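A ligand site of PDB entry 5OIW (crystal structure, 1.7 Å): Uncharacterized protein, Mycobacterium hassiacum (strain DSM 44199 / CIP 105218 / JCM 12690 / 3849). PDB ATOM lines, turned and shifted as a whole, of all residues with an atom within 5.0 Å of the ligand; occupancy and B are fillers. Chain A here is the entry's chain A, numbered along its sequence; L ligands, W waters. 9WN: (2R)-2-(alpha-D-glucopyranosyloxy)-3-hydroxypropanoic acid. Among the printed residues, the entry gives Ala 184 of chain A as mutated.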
ATOM      1  N   ALA A  33     -26.025   0.491 -14.337  1.00  0.00           N
ATOM      2  CA  ALA A  33     -26.322   1.903 -14.506  1.00  0.00           C
ATOM      3  C   ALA A  33     -27.784   2.108 -14.916  1.00  0.00           C
ATOM      4  O   ALA A  33     -28.365   3.158 -14.629  1.00  0.00           O
ATOM      5  CB  ALA A  33     -25.364   2.532 -15.561  1.00  0.00           C
ATOM      6  N   TYR A  38     -28.099  -0.126 -20.009  1.00  0.00           N
ATOM      7  CA  TYR A  38     -26.757  -0.129 -19.448  1.00  0.00           C
ATOM      8  C   TYR A  38     -26.672  -1.204 -18.378  1.00  0.00           C
ATOM      9  O   TYR A  38     -26.573  -0.894 -17.181  1.00  0.00           O
ATOM     10  CB  TYR A  38     -26.433   1.241 -18.836  1.00  0.00           C
ATOM     11  CG  TYR A  38     -26.551   2.425 -19.787  1.00  0.00           C
ATOM     12  CD1 TYR A  38     -25.806   2.485 -20.953  1.00  0.00           C
ATOM     13  CD2 TYR A  38     -27.374   3.518 -19.469  1.00  0.00           C
ATOM     14  CE1 TYR A  38     -25.906   3.592 -21.819  1.00  0.00           C
ATOM     15  CE2 TYR A  38     -27.463   4.638 -20.303  1.00  0.00           C
ATOM     16  CZ  TYR A  38     -26.730   4.664 -21.480  1.00  0.00           C
ATOM     17  OH  TYR A  38     -26.839   5.761 -22.305  1.00  0.00           O
ATOM     18  N   TRP A  42     -20.855   0.911 -14.755  1.00  0.00           N
ATOM     19  CA  TRP A  42     -20.038   1.979 -15.325  1.00  0.00           C
ATOM     20  C   TRP A  42     -19.298   2.716 -14.227  1.00  0.00           C
ATOM     21  O   TRP A  42     -19.770   2.805 -13.089  1.00  0.00           O
ATOM     22  CB  TRP A  42     -20.884   2.987 -16.115  1.00  0.00           C
ATOM     23  CG  TRP A  42     -20.974   2.718 -17.609  1.00  0.00           C
ATOM     24  CD1 TRP A  42     -20.357   3.404 -18.610  1.00  0.00           C
ATOM     25  CD2 TRP A  42     -21.756   1.683 -18.239  1.00  0.00           C
ATOM     26  NE1 TRP A  42     -20.707   2.873 -19.834  1.00  0.00           N
ATOM     27  CE2 TRP A  42     -21.546   1.800 -19.634  1.00  0.00           C
ATOM     28  CE3 TRP A  42     -22.586   0.652 -17.764  1.00  0.00           C
ATOM     29  CZ2 TRP A  42     -22.138   0.937 -20.565  1.00  0.00           C
ATOM     30  CZ3 TRP A  42     -23.181  -0.219 -18.707  1.00  0.00           C
ATOM     31  CH2 TRP A  42     -22.951  -0.063 -20.096  1.00  0.00           C
ATOM     32  N   TRP A  44     -18.038   6.104 -13.634  1.00  0.00           N
ATOM     33  CA  TRP A  44     -18.457   7.273 -12.868  1.00  0.00           C
ATOM     34  C   TRP A  44     -19.892   7.106 -12.375  1.00  0.00           C
ATOM     35  O   TRP A  44     -20.197   7.562 -11.272  1.00  0.00           O
ATOM     36  CB  TRP A  44     -18.223   8.622 -13.613  1.00  0.00           C
ATOM     37  CG  TRP A  44     -19.004   9.064 -14.835  1.00  0.00           C
ATOM     38  CD1 TRP A  44     -19.615   8.303 -15.806  1.00  0.00           C
ATOM     39  CD2 TRP A  44     -19.215  10.434 -15.210  1.00  0.00           C
ATOM     40  NE1 TRP A  44     -20.188   9.122 -16.765  1.00  0.00           N
ATOM     41  CE2 TRP A  44     -19.973  10.441 -16.409  1.00  0.00           C
ATOM     42  CE3 TRP A  44     -18.822  11.656 -14.651  1.00  0.00           C
ATOM     43  CZ2 TRP A  44     -20.342  11.626 -17.056  1.00  0.00           C
ATOM     44  CZ3 TRP A  44     -19.227  12.840 -15.272  1.00  0.00           C
ATOM     45  CH2 TRP A  44     -19.971  12.820 -16.475  1.00  0.00           C
ATOM     46  N   ASP A  45     -20.715   6.286 -13.058  1.00  0.00           N
ATOM     47  CA  ASP A  45     -22.024   5.950 -12.477  1.00  0.00           C
ATOM     48  C   ASP A  45     -21.860   5.269 -11.125  1.00  0.00           C
ATOM     49  O   ASP A  45     -22.650   5.527 -10.199  1.00  0.00           O
ATOM     50  CB  ASP A  45     -22.847   5.006 -13.371  1.00  0.00           C
ATOM     51  CG  ASP A  45     -23.117   5.581 -14.744  1.00  0.00           C
ATOM     52  OD1 ASP A  45     -22.109   5.936 -15.417  1.00  0.00           O
ATOM     53  OD2 ASP A  45     -24.321   5.685 -15.171  1.00  0.00           O
ATOM     54  N   HIS A  80     -13.954   2.055 -17.793  1.00  0.00           N
ATOM     55  CA  HIS A  80     -15.234   2.722 -17.657  1.00  0.00           C
ATOM     56  C   HIS A  80     -16.399   1.758 -17.590  1.00  0.00           C
ATOM     57  O   HIS A  80     -17.465   2.179 -17.120  1.00  0.00           O
ATOM     58  CB  HIS A  80     -15.445   3.772 -18.766  1.00  0.00           C
ATOM     59  CG  HIS A  80     -16.092   3.271 -20.022  1.00  0.00           C
ATOM     60  ND1 HIS A  80     -15.578   2.248 -20.789  1.00  0.00           N
ATOM     61  CD2 HIS A  80     -17.160   3.755 -20.720  1.00  0.00           C
ATOM     62  CE1 HIS A  80     -16.331   2.073 -21.854  1.00  0.00           C
ATOM     63  NE2 HIS A  80     -17.287   2.985 -21.851  1.00  0.00           N
ATOM     64  N   TYR A  90     -25.711  -5.108 -24.239  1.00  0.00           N
ATOM     65  CA  TYR A  90     -25.003  -3.852 -24.433  1.00  0.00           C
ATOM     66  C   TYR A  90     -23.931  -4.053 -25.485  1.00  0.00           C
ATOM     67  O   TYR A  90     -23.227  -5.053 -25.451  1.00  0.00           O
ATOM     68  CB  TYR A  90     -24.331  -3.351 -23.158  1.00  0.00           C
ATOM     69  CG  TYR A  90     -23.567  -2.074 -23.413  1.00  0.00           C
ATOM     70  CD1 TYR A  90     -24.243  -0.858 -23.449  1.00  0.00           C
ATOM     71  CD2 TYR A  90     -22.206  -2.077 -23.675  1.00  0.00           C
ATOM     72  CE1 TYR A  90     -23.582   0.304 -23.728  1.00  0.00           C
ATOM     73  CE2 TYR A  90     -21.545  -0.914 -23.929  1.00  0.00           C
ATOM     74  CZ  TYR A  90     -22.219   0.272 -23.948  1.00  0.00           C
ATOM     75  OH  TYR A  90     -21.559   1.449 -24.235  1.00  0.00           O
ATOM     76  N   GLN A 117     -12.866   6.865 -17.481  1.00  0.00           N
ATOM     77  CA  GLN A 117     -13.988   7.780 -17.271  1.00  0.00           C
ATOM     78  C   GLN A 117     -13.636   8.733 -16.127  1.00  0.00           C
ATOM     79  O   GLN A 117     -12.659   8.508 -15.412  1.00  0.00           O
ATOM     80  CB  GLN A 117     -15.286   6.997 -16.961  1.00  0.00           C
ATOM     81  CG  GLN A 117     -16.322   7.130 -18.087  1.00  0.00           C
ATOM     82  CD  GLN A 117     -17.670   6.512 -17.696  1.00  0.00           C
ATOM     83  OE1 GLN A 117     -17.811   5.932 -16.603  1.00  0.00           O
ATOM     84  NE2 GLN A 117     -18.665   6.644 -18.578  1.00  0.00           N
ATOM     85  N   TRP A 179     -15.820   8.715 -25.358  1.00  0.00           N
ATOM     86  CA  TRP A 179     -16.520   8.049 -24.257  1.00  0.00           C
ATOM     87  C   TRP A 179     -15.836   8.272 -22.909  1.00  0.00           C
ATOM     88  O   TRP A 179     -16.500   8.191 -21.868  1.00  0.00           O
ATOM     89  CB  TRP A 179     -16.649   6.539 -24.526  1.00  0.00           C
ATOM     90  CG  TRP A 179     -17.782   6.131 -25.453  1.00  0.00           C
ATOM     91  CD1 TRP A 179     -18.970   6.799 -25.643  1.00  0.00           C
ATOM     92  CD2 TRP A 179     -17.850   4.960 -26.271  1.00  0.00           C
ATOM     93  NE1 TRP A 179     -19.769   6.094 -26.545  1.00  0.00           N
ATOM     94  CE2 TRP A 179     -19.096   4.960 -26.937  1.00  0.00           C
ATOM     95  CE3 TRP A 179     -16.963   3.886 -26.506  1.00  0.00           C
ATOM     96  CZ2 TRP A 179     -19.495   3.948 -27.824  1.00  0.00           C
ATOM     97  CZ3 TRP A 179     -17.343   2.875 -27.381  1.00  0.00           C
ATOM     98  CH2 TRP A 179     -18.601   2.911 -28.032  1.00  0.00           C
ATOM     99  N   GLY A 182     -17.276  10.941 -20.658  1.00  0.00           N
ATOM    100  CA  GLY A 182     -18.649  10.748 -20.216  1.00  0.00           C
ATOM    101  C   GLY A 182     -19.710  11.298 -21.166  1.00  0.00           C
ATOM    102  O   GLY A 182     -20.897  11.003 -20.976  1.00  0.00           O
ATOM    103  N   MET A 183     -19.317  12.048 -22.194  1.00  0.00           N
ATOM    104  CA  MET A 183     -20.273  12.784 -23.046  1.00  0.00           C
ATOM    105  C   MET A 183     -20.040  12.387 -24.497  1.00  0.00           C
ATOM    106  O   MET A 183     -19.492  13.177 -25.291  1.00  0.00           O
ATOM    107  CB  MET A 183     -20.104  14.291 -22.843  1.00  0.00           C
ATOM    108  CG  MET A 183     -20.141  14.703 -21.355  1.00  0.00           C
ATOM    109  SD  MET A 183     -20.134  16.537 -21.320  1.00  0.00           S
ATOM    110  CE  MET A 183     -19.974  16.782 -19.558  1.00  0.00           C
ATOM    111  N   ALA A 184     -20.499  11.192 -24.854  1.00  0.00           N
ATOM    112  CA  ALA A 184     -20.189  10.573 -26.155  1.00  0.00           C
ATOM    113  C   ALA A 184     -20.301  11.530 -27.341  1.00  0.00           C
ATOM    114  O   ALA A 184     -19.374  11.650 -28.165  1.00  0.00           O
ATOM    115  CB  ALA A 184     -21.136   9.378 -26.388  1.00  0.00           C
ATOM    116  N   ARG A 218     -30.430   9.330 -29.587  1.00  0.00           N
ATOM    117  CA  ARG A 218     -29.138   8.655 -29.535  1.00  0.00           C
ATOM    118  C   ARG A 218     -28.247   9.138 -30.672  1.00  0.00           C
ATOM    119  O   ARG A 218     -28.727   9.736 -31.629  1.00  0.00           O
ATOM    120  CB  ARG A 218     -29.277   7.121 -29.627  1.00  0.00           C
ATOM    121  CG  ARG A 218     -30.136   6.505 -28.502  1.00  0.00           C
ATOM    122  CD  ARG A 218     -29.396   6.406 -27.183  1.00  0.00           C
ATOM    123  NE  ARG A 218     -28.068   5.770 -27.274  1.00  0.00           N
ATOM    124  CZ  ARG A 218     -27.219   5.683 -26.241  1.00  0.00           C
ATOM    125  NH1 ARG A 218     -27.557   6.194 -25.053  1.00  0.00           N
ATOM    126  NH2 ARG A 218     -26.034   5.094 -26.394  1.00  0.00           N
ATOM    127  N   TYR A 224     -21.252   6.206 -34.359  1.00  0.00           N
ATOM    128  CA  TYR A 224     -20.845   4.911 -33.823  1.00  0.00           C
ATOM    129  C   TYR A 224     -19.708   4.295 -34.631  1.00  0.00           C
ATOM    130  O   TYR A 224     -18.822   3.636 -34.062  1.00  0.00           O
ATOM    131  CB  TYR A 224     -22.044   3.952 -33.742  1.00  0.00           C
ATOM    132  CG  TYR A 224     -22.606   3.914 -32.355  1.00  0.00           C
ATOM    133  CD1 TYR A 224     -23.441   4.945 -31.879  1.00  0.00           C
ATOM    134  CD2 TYR A 224     -22.238   2.901 -31.474  1.00  0.00           C
ATOM    135  CE1 TYR A 224     -23.921   4.934 -30.569  1.00  0.00           C
ATOM    136  CE2 TYR A 224     -22.725   2.870 -30.150  1.00  0.00           C
ATOM    137  CZ  TYR A 224     -23.549   3.902 -29.720  1.00  0.00           C
ATOM    138  OH  TYR A 224     -24.005   3.890 -28.415  1.00  0.00           O
ATOM    139  N   TYR A 377     -29.327  13.476 -26.531  1.00  0.00           N
ATOM    140  CA  TYR A 377     -28.302  12.912 -25.656  1.00  0.00           C
ATOM    141  C   TYR A 377     -27.453  14.015 -24.999  1.00  0.00           C
ATOM    142  O   TYR A 377     -27.939  14.696 -24.107  1.00  0.00           O
ATOM    143  CB  TYR A 377     -27.492  11.915 -26.493  1.00  0.00           C
ATOM    144  CG  TYR A 377     -26.651  10.849 -25.811  1.00  0.00           C
ATOM    145  CD1 TYR A 377     -26.964  10.347 -24.555  1.00  0.00           C
ATOM    146  CD2 TYR A 377     -25.566  10.305 -26.481  1.00  0.00           C
ATOM    147  CE1 TYR A 377     -26.173   9.354 -23.972  1.00  0.00           C
ATOM    148  CE2 TYR A 377     -24.784   9.337 -25.911  1.00  0.00           C
ATOM    149  CZ  TYR A 377     -25.090   8.854 -24.669  1.00  0.00           C
ATOM    150  OH  TYR A 377     -24.276   7.894 -24.145  1.00  0.00           O
ATOM    151  N   TRP A 378     -26.193  14.218 -25.421  1.00  0.00           N
ATOM    152  CA  TRP A 378     -25.383  15.285 -24.842  1.00  0.00           C
ATOM    153  C   TRP A 378     -25.414  16.582 -25.645  1.00  0.00           C
ATOM    154  O   TRP A 378     -24.675  17.517 -25.316  1.00  0.00           O
ATOM    155  CB  TRP A 378     -23.921  14.835 -24.655  1.00  0.00           C
ATOM    156  CG  TRP A 378     -23.763  13.805 -23.528  1.00  0.00           C
ATOM    157  CD1 TRP A 378     -23.711  12.448 -23.672  1.00  0.00           C
ATOM    158  CD2 TRP A 378     -23.708  14.067 -22.123  1.00  0.00           C
ATOM    159  NE1 TRP A 378     -23.592  11.852 -22.420  1.00  0.00           N
ATOM    160  CE2 TRP A 378     -23.590  12.814 -21.459  1.00  0.00           C
ATOM    161  CE3 TRP A 378     -23.733  15.239 -21.351  1.00  0.00           C
ATOM    162  CZ2 TRP A 378     -23.480  12.712 -20.040  1.00  0.00           C
ATOM    163  CZ3 TRP A 378     -23.646  15.143 -19.963  1.00  0.00           C
ATOM    164  CH2 TRP A 378     -23.508  13.897 -19.326  1.00  0.00           C
ATOM    165  N   TRP A 383     -29.182  16.860 -17.818  1.00  0.00           N
ATOM    166  CA  TRP A 383     -28.791  15.600 -17.164  1.00  0.00           C
ATOM    167  C   TRP A 383     -28.821  15.755 -15.657  1.00  0.00           C
ATOM    168  O   TRP A 383     -28.060  16.582 -15.115  1.00  0.00           O
ATOM    169  CB  TRP A 383     -27.388  15.210 -17.607  1.00  0.00           C
ATOM    170  CG  TRP A 383     -27.323  14.733 -19.003  1.00  0.00           C
ATOM    171  CD1 TRP A 383     -27.488  15.472 -20.145  1.00  0.00           C
ATOM    172  CD2 TRP A 383     -27.063  13.392 -19.417  1.00  0.00           C
ATOM    173  NE1 TRP A 383     -27.370  14.646 -21.251  1.00  0.00           N
ATOM    174  CE2 TRP A 383     -27.084  13.381 -20.822  1.00  0.00           C
ATOM    175  CE3 TRP A 383     -26.810  12.191 -18.715  1.00  0.00           C
ATOM    176  CZ2 TRP A 383     -26.860  12.215 -21.561  1.00  0.00           C
ATOM    177  CZ3 TRP A 383     -26.594  11.035 -19.458  1.00  0.00           C
ATOM    178  CH2 TRP A 383     -26.598  11.055 -20.870  1.00  0.00           C
ATOM    179  N   GLU A 421     -32.682   9.282 -17.543  1.00  0.00           N
ATOM    180  CA  GLU A 421     -31.269   9.545 -17.826  1.00  0.00           C
ATOM    181  C   GLU A 421     -31.022  11.026 -18.132  1.00  0.00           C
ATOM    182  O   GLU A 421     -30.047  11.616 -17.641  1.00  0.00           O
ATOM    183  CB  GLU A 421     -30.876   8.654 -19.017  1.00  0.00           C
ATOM    184  CG  GLU A 421     -29.374   8.568 -19.321  1.00  0.00           C
ATOM    185  CD  GLU A 421     -29.094   7.795 -20.606  1.00  0.00           C
ATOM    186  OE1 GLU A 421     -30.044   7.234 -21.222  1.00  0.00           O
ATOM    187  OE2 GLU A 421     -27.912   7.712 -21.005  1.00  0.00           O
ATOM    188  N   GLN A 436     -32.796   5.189 -14.328  1.00  0.00           N
ATOM    189  CA  GLN A 436     -31.354   5.370 -14.400  1.00  0.00           C
ATOM    190  C   GLN A 436     -30.790   5.527 -12.992  1.00  0.00           C
ATOM    191  O   GLN A 436     -31.223   6.400 -12.237  1.00  0.00           O
ATOM    192  CB  GLN A 436     -31.066   6.618 -15.242  1.00  0.00           C
ATOM    193  CG  GLN A 436     -29.561   6.896 -15.488  1.00  0.00           C
ATOM    194  CD  GLN A 436     -28.953   6.001 -16.583  1.00  0.00           C
ATOM    195  OE1 GLN A 436     -29.662   5.383 -17.357  1.00  0.00           O
ATOM    196  NE2 GLN A 436     -27.610   5.970 -16.639  1.00  0.00           N
ATOM    197  N   TRP A 438     -27.982   6.676 -11.520  1.00  0.00           N
ATOM    198  CA  TRP A 438     -27.431   7.874 -10.917  1.00  0.00           C
ATOM    199  C   TRP A 438     -28.453   9.005 -10.786  1.00  0.00           C
ATOM    200  O   TRP A 438     -28.252   9.932  -9.987  1.00  0.00           O
ATOM    201  CB  TRP A 438     -26.152   8.323 -11.678  1.00  0.00           C
ATOM    202  CG  TRP A 438     -26.263   8.711 -13.101  1.00  0.00           C
ATOM    203  CD1 TRP A 438     -27.386   8.941 -13.860  1.00  0.00           C
ATOM    204  CD2 TRP A 438     -25.133   8.937 -13.962  1.00  0.00           C
ATOM    205  NE1 TRP A 438     -27.009   9.282 -15.168  1.00  0.00           N
ATOM    206  CE2 TRP A 438     -25.634   9.291 -15.239  1.00  0.00           C
ATOM    207  CE3 TRP A 438     -23.758   8.894 -13.756  1.00  0.00           C
ATOM    208  CZ2 TRP A 438     -24.788   9.576 -16.320  1.00  0.00           C
ATOM    209  CZ3 TRP A 438     -22.920   9.190 -14.817  1.00  0.00           C
ATOM    210  CH2 TRP A 438     -23.437   9.483 -16.095  1.00  0.00           C
HETATM  211  C10 9WN L   1     -20.823   4.730 -23.115  1.00  0.00           C
HETATM  212  C6  9WN L   1     -23.749   4.753 -18.251  1.00  0.00           C
HETATM  213  C5  9WN L   1     -23.023   5.629 -19.317  1.00  0.00           C
HETATM  214  C4  9WN L   1     -22.655   6.983 -18.714  1.00  0.00           C
HETATM  215  C3  9WN L   1     -22.300   7.938 -19.799  1.00  0.00           C
HETATM  216  C2  9WN L   1     -23.374   8.045 -20.815  1.00  0.00           C
HETATM  217  C1  9WN L   1     -23.588   6.679 -21.480  1.00  0.00           C
HETATM  218  C09 9WN L   1     -22.296   4.961 -22.729  1.00  0.00           C
HETATM  219  C12 9WN L   1     -23.166   4.675 -23.969  1.00  0.00           C
HETATM  220  O5  9WN L   1     -23.929   5.700 -20.461  1.00  0.00           O
HETATM  221  O1  9WN L   1     -22.421   6.261 -22.196  1.00  0.00           O
HETATM  222  O11 9WN L   1     -20.012   4.685 -21.973  1.00  0.00           O
HETATM  223  O13 9WN L   1     -23.840   5.567 -24.543  1.00  0.00           O
HETATM  224  O14 9WN L   1     -23.172   3.500 -24.445  1.00  0.00           O
HETATM  225  O2  9WN L   1     -23.068   8.977 -21.832  1.00  0.00           O
HETATM  226  O3  9WN L   1     -21.986   9.195 -19.251  1.00  0.00           O
HETATM  227  O4  9WN L   1     -21.542   6.738 -17.877  1.00  0.00           O
HETATM  228  O6  9WN L   1     -24.870   5.433 -17.790  1.00  0.00           O
HETATM  229  O   HOH W   1     -19.008   7.314 -21.535  1.00  0.00           O
HETATM  230  O   HOH W   2     -26.143   7.699 -18.860  1.00  0.00           O
HETATM  231  O   HOH W   3     -20.828   8.698 -23.172  1.00  0.00           O
HETATM  232  O   HOH W   4     -23.695   1.964 -26.740  1.00  0.00           O
HETATM  233  O   HOH W   5     -22.668   6.424 -27.137  1.00  0.00           O
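Water W3 lies within hydrogen-bond range of an oxygen (O2) of the ligand (2.6 Å), the backbone NH of Ala 184 (3.0 Å) and the backbone carbonyl oxygen of Gly 182 (3.2 Å). Water W2 lies within hydrogen-bond range of OE2 of Glu 421 (2.8 Å), O6 of the ligand (2.8 Å) and NE2 of Gln 436 (3.2 Å). Water W4 lies within hydrogen-bond range of the side-chain hydroxyl of Tyr 224 (2.6 Å), an oxygen (O14) of the ligand (2.8 Å) and the side-chain hydroxyl of Tyr 90 (3.3 Å). Water W1 lies within hydrogen-bond range of O of Trp 179, O11 of the ligand and NE2 of Gln 117. Water W5 lies within hydrogen-bond range of an oxygen (O13) of the ligand (3.0 Å), the indole nitrogen (NE1) of Trp 179 (3.0 Å) and the side-chain hydroxyl (OH) of Tyr 224 (3.1 Å).
The side-chain carboxylate of Glu 421 lies within hydrogen-bond range of the side-chain hydroxyl of Tyr 38 (2.6 Å). The side-chain amide oxygen (OE1) of Gln 117 sits at hydrogen-bond distance from the backbone NH (N) of Trp 44, 3.0 Å away. N of Ala 33 sits at hydrogen-bond distance from O of Tyr 38. The backbone carbonyl oxygen (O) of Gly 182 is in hydrogen-bond range of the indole nitrogen (NE1) of Trp 378, at 3.2 Å. NH1 of Arg 218 lies within hydrogen-bond range of OH of Tyr 38 (2.9 Å). The side-chain hydroxyl of Tyr 224 lies within hydrogen-bond range of the guanidinium group of Arg 218, at 3.1 Å. The indole nitrogen of Trp 383 is in hydrogen-bond range of the backbone carbonyl oxygen of Tyr 377 (2.9 Å).
Ala 33 touches the ligand (CB to O6, 3.7 Å). Trp 179 touches the ligand. Trp 438 touches the ligand. Hydrophobic or aromatic side chains that line the ligand: Ala 33, Tyr 38, Trp 42, Trp 44, His 80, Tyr 90, Trp 179, Tyr 377, Trp 378 and Trp 438. 15 residues have an atom within 4 Å of the ligand: Ala 33, Tyr 38, Trp 42, Trp 44, Asp 45, His 80, Tyr 90, Gln 117, Trp 179, Gly 182, Arg 218, Tyr 377, Trp 378, Gln 436 and Trp 438.
An oxygen (O5) of the ligand sits close to the side-chain hydroxyl of Tyr 38 (3.4 Å). An oxygen (O2) of the ligand is in hydrogen-bond range of the indole nitrogen (NE1) of Trp 378, 3.0 Å away. NE1 of Trp 42 sits at hydrogen-bond distance from O11 of the ligand (2.9 Å). NE2 of Gln 117 is in hydrogen-bond range of O4 of the ligand (3.0 Å). NE2 of Gln 436 is in hydrogen-bond range of O6 of the ligand (3.0 Å). The side-chain hydroxyl (OH) of Tyr 377 sits at hydrogen-bond distance from an oxygen (O13) of the ligand (2.4 Å). A ring nitrogen (NE2) of His 80 lies within hydrogen-bond range of an oxygen (O11) of the ligand (3.2 Å). The indole nitrogen of Trp 44 sits at hydrogen-bond distance from an oxygen (O4) of the ligand, at 3.0 Å. The side-chain carboxylate of Asp 45 sits at hydrogen-bond distance from an oxygen (O4) of the ligand, 2.6 Å away. An oxygen (O14) of the ligand lies within hydrogen-bond range of the side-chain hydroxyl (OH) of Tyr 90. An oxygen (O13) of the ligand lies within salt-bridge range of the guanidinium group of Arg 218 (2.9 Å). O of Gly 182 sits at hydrogen-bond distance from O3 of the ligand (2.7 Å).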
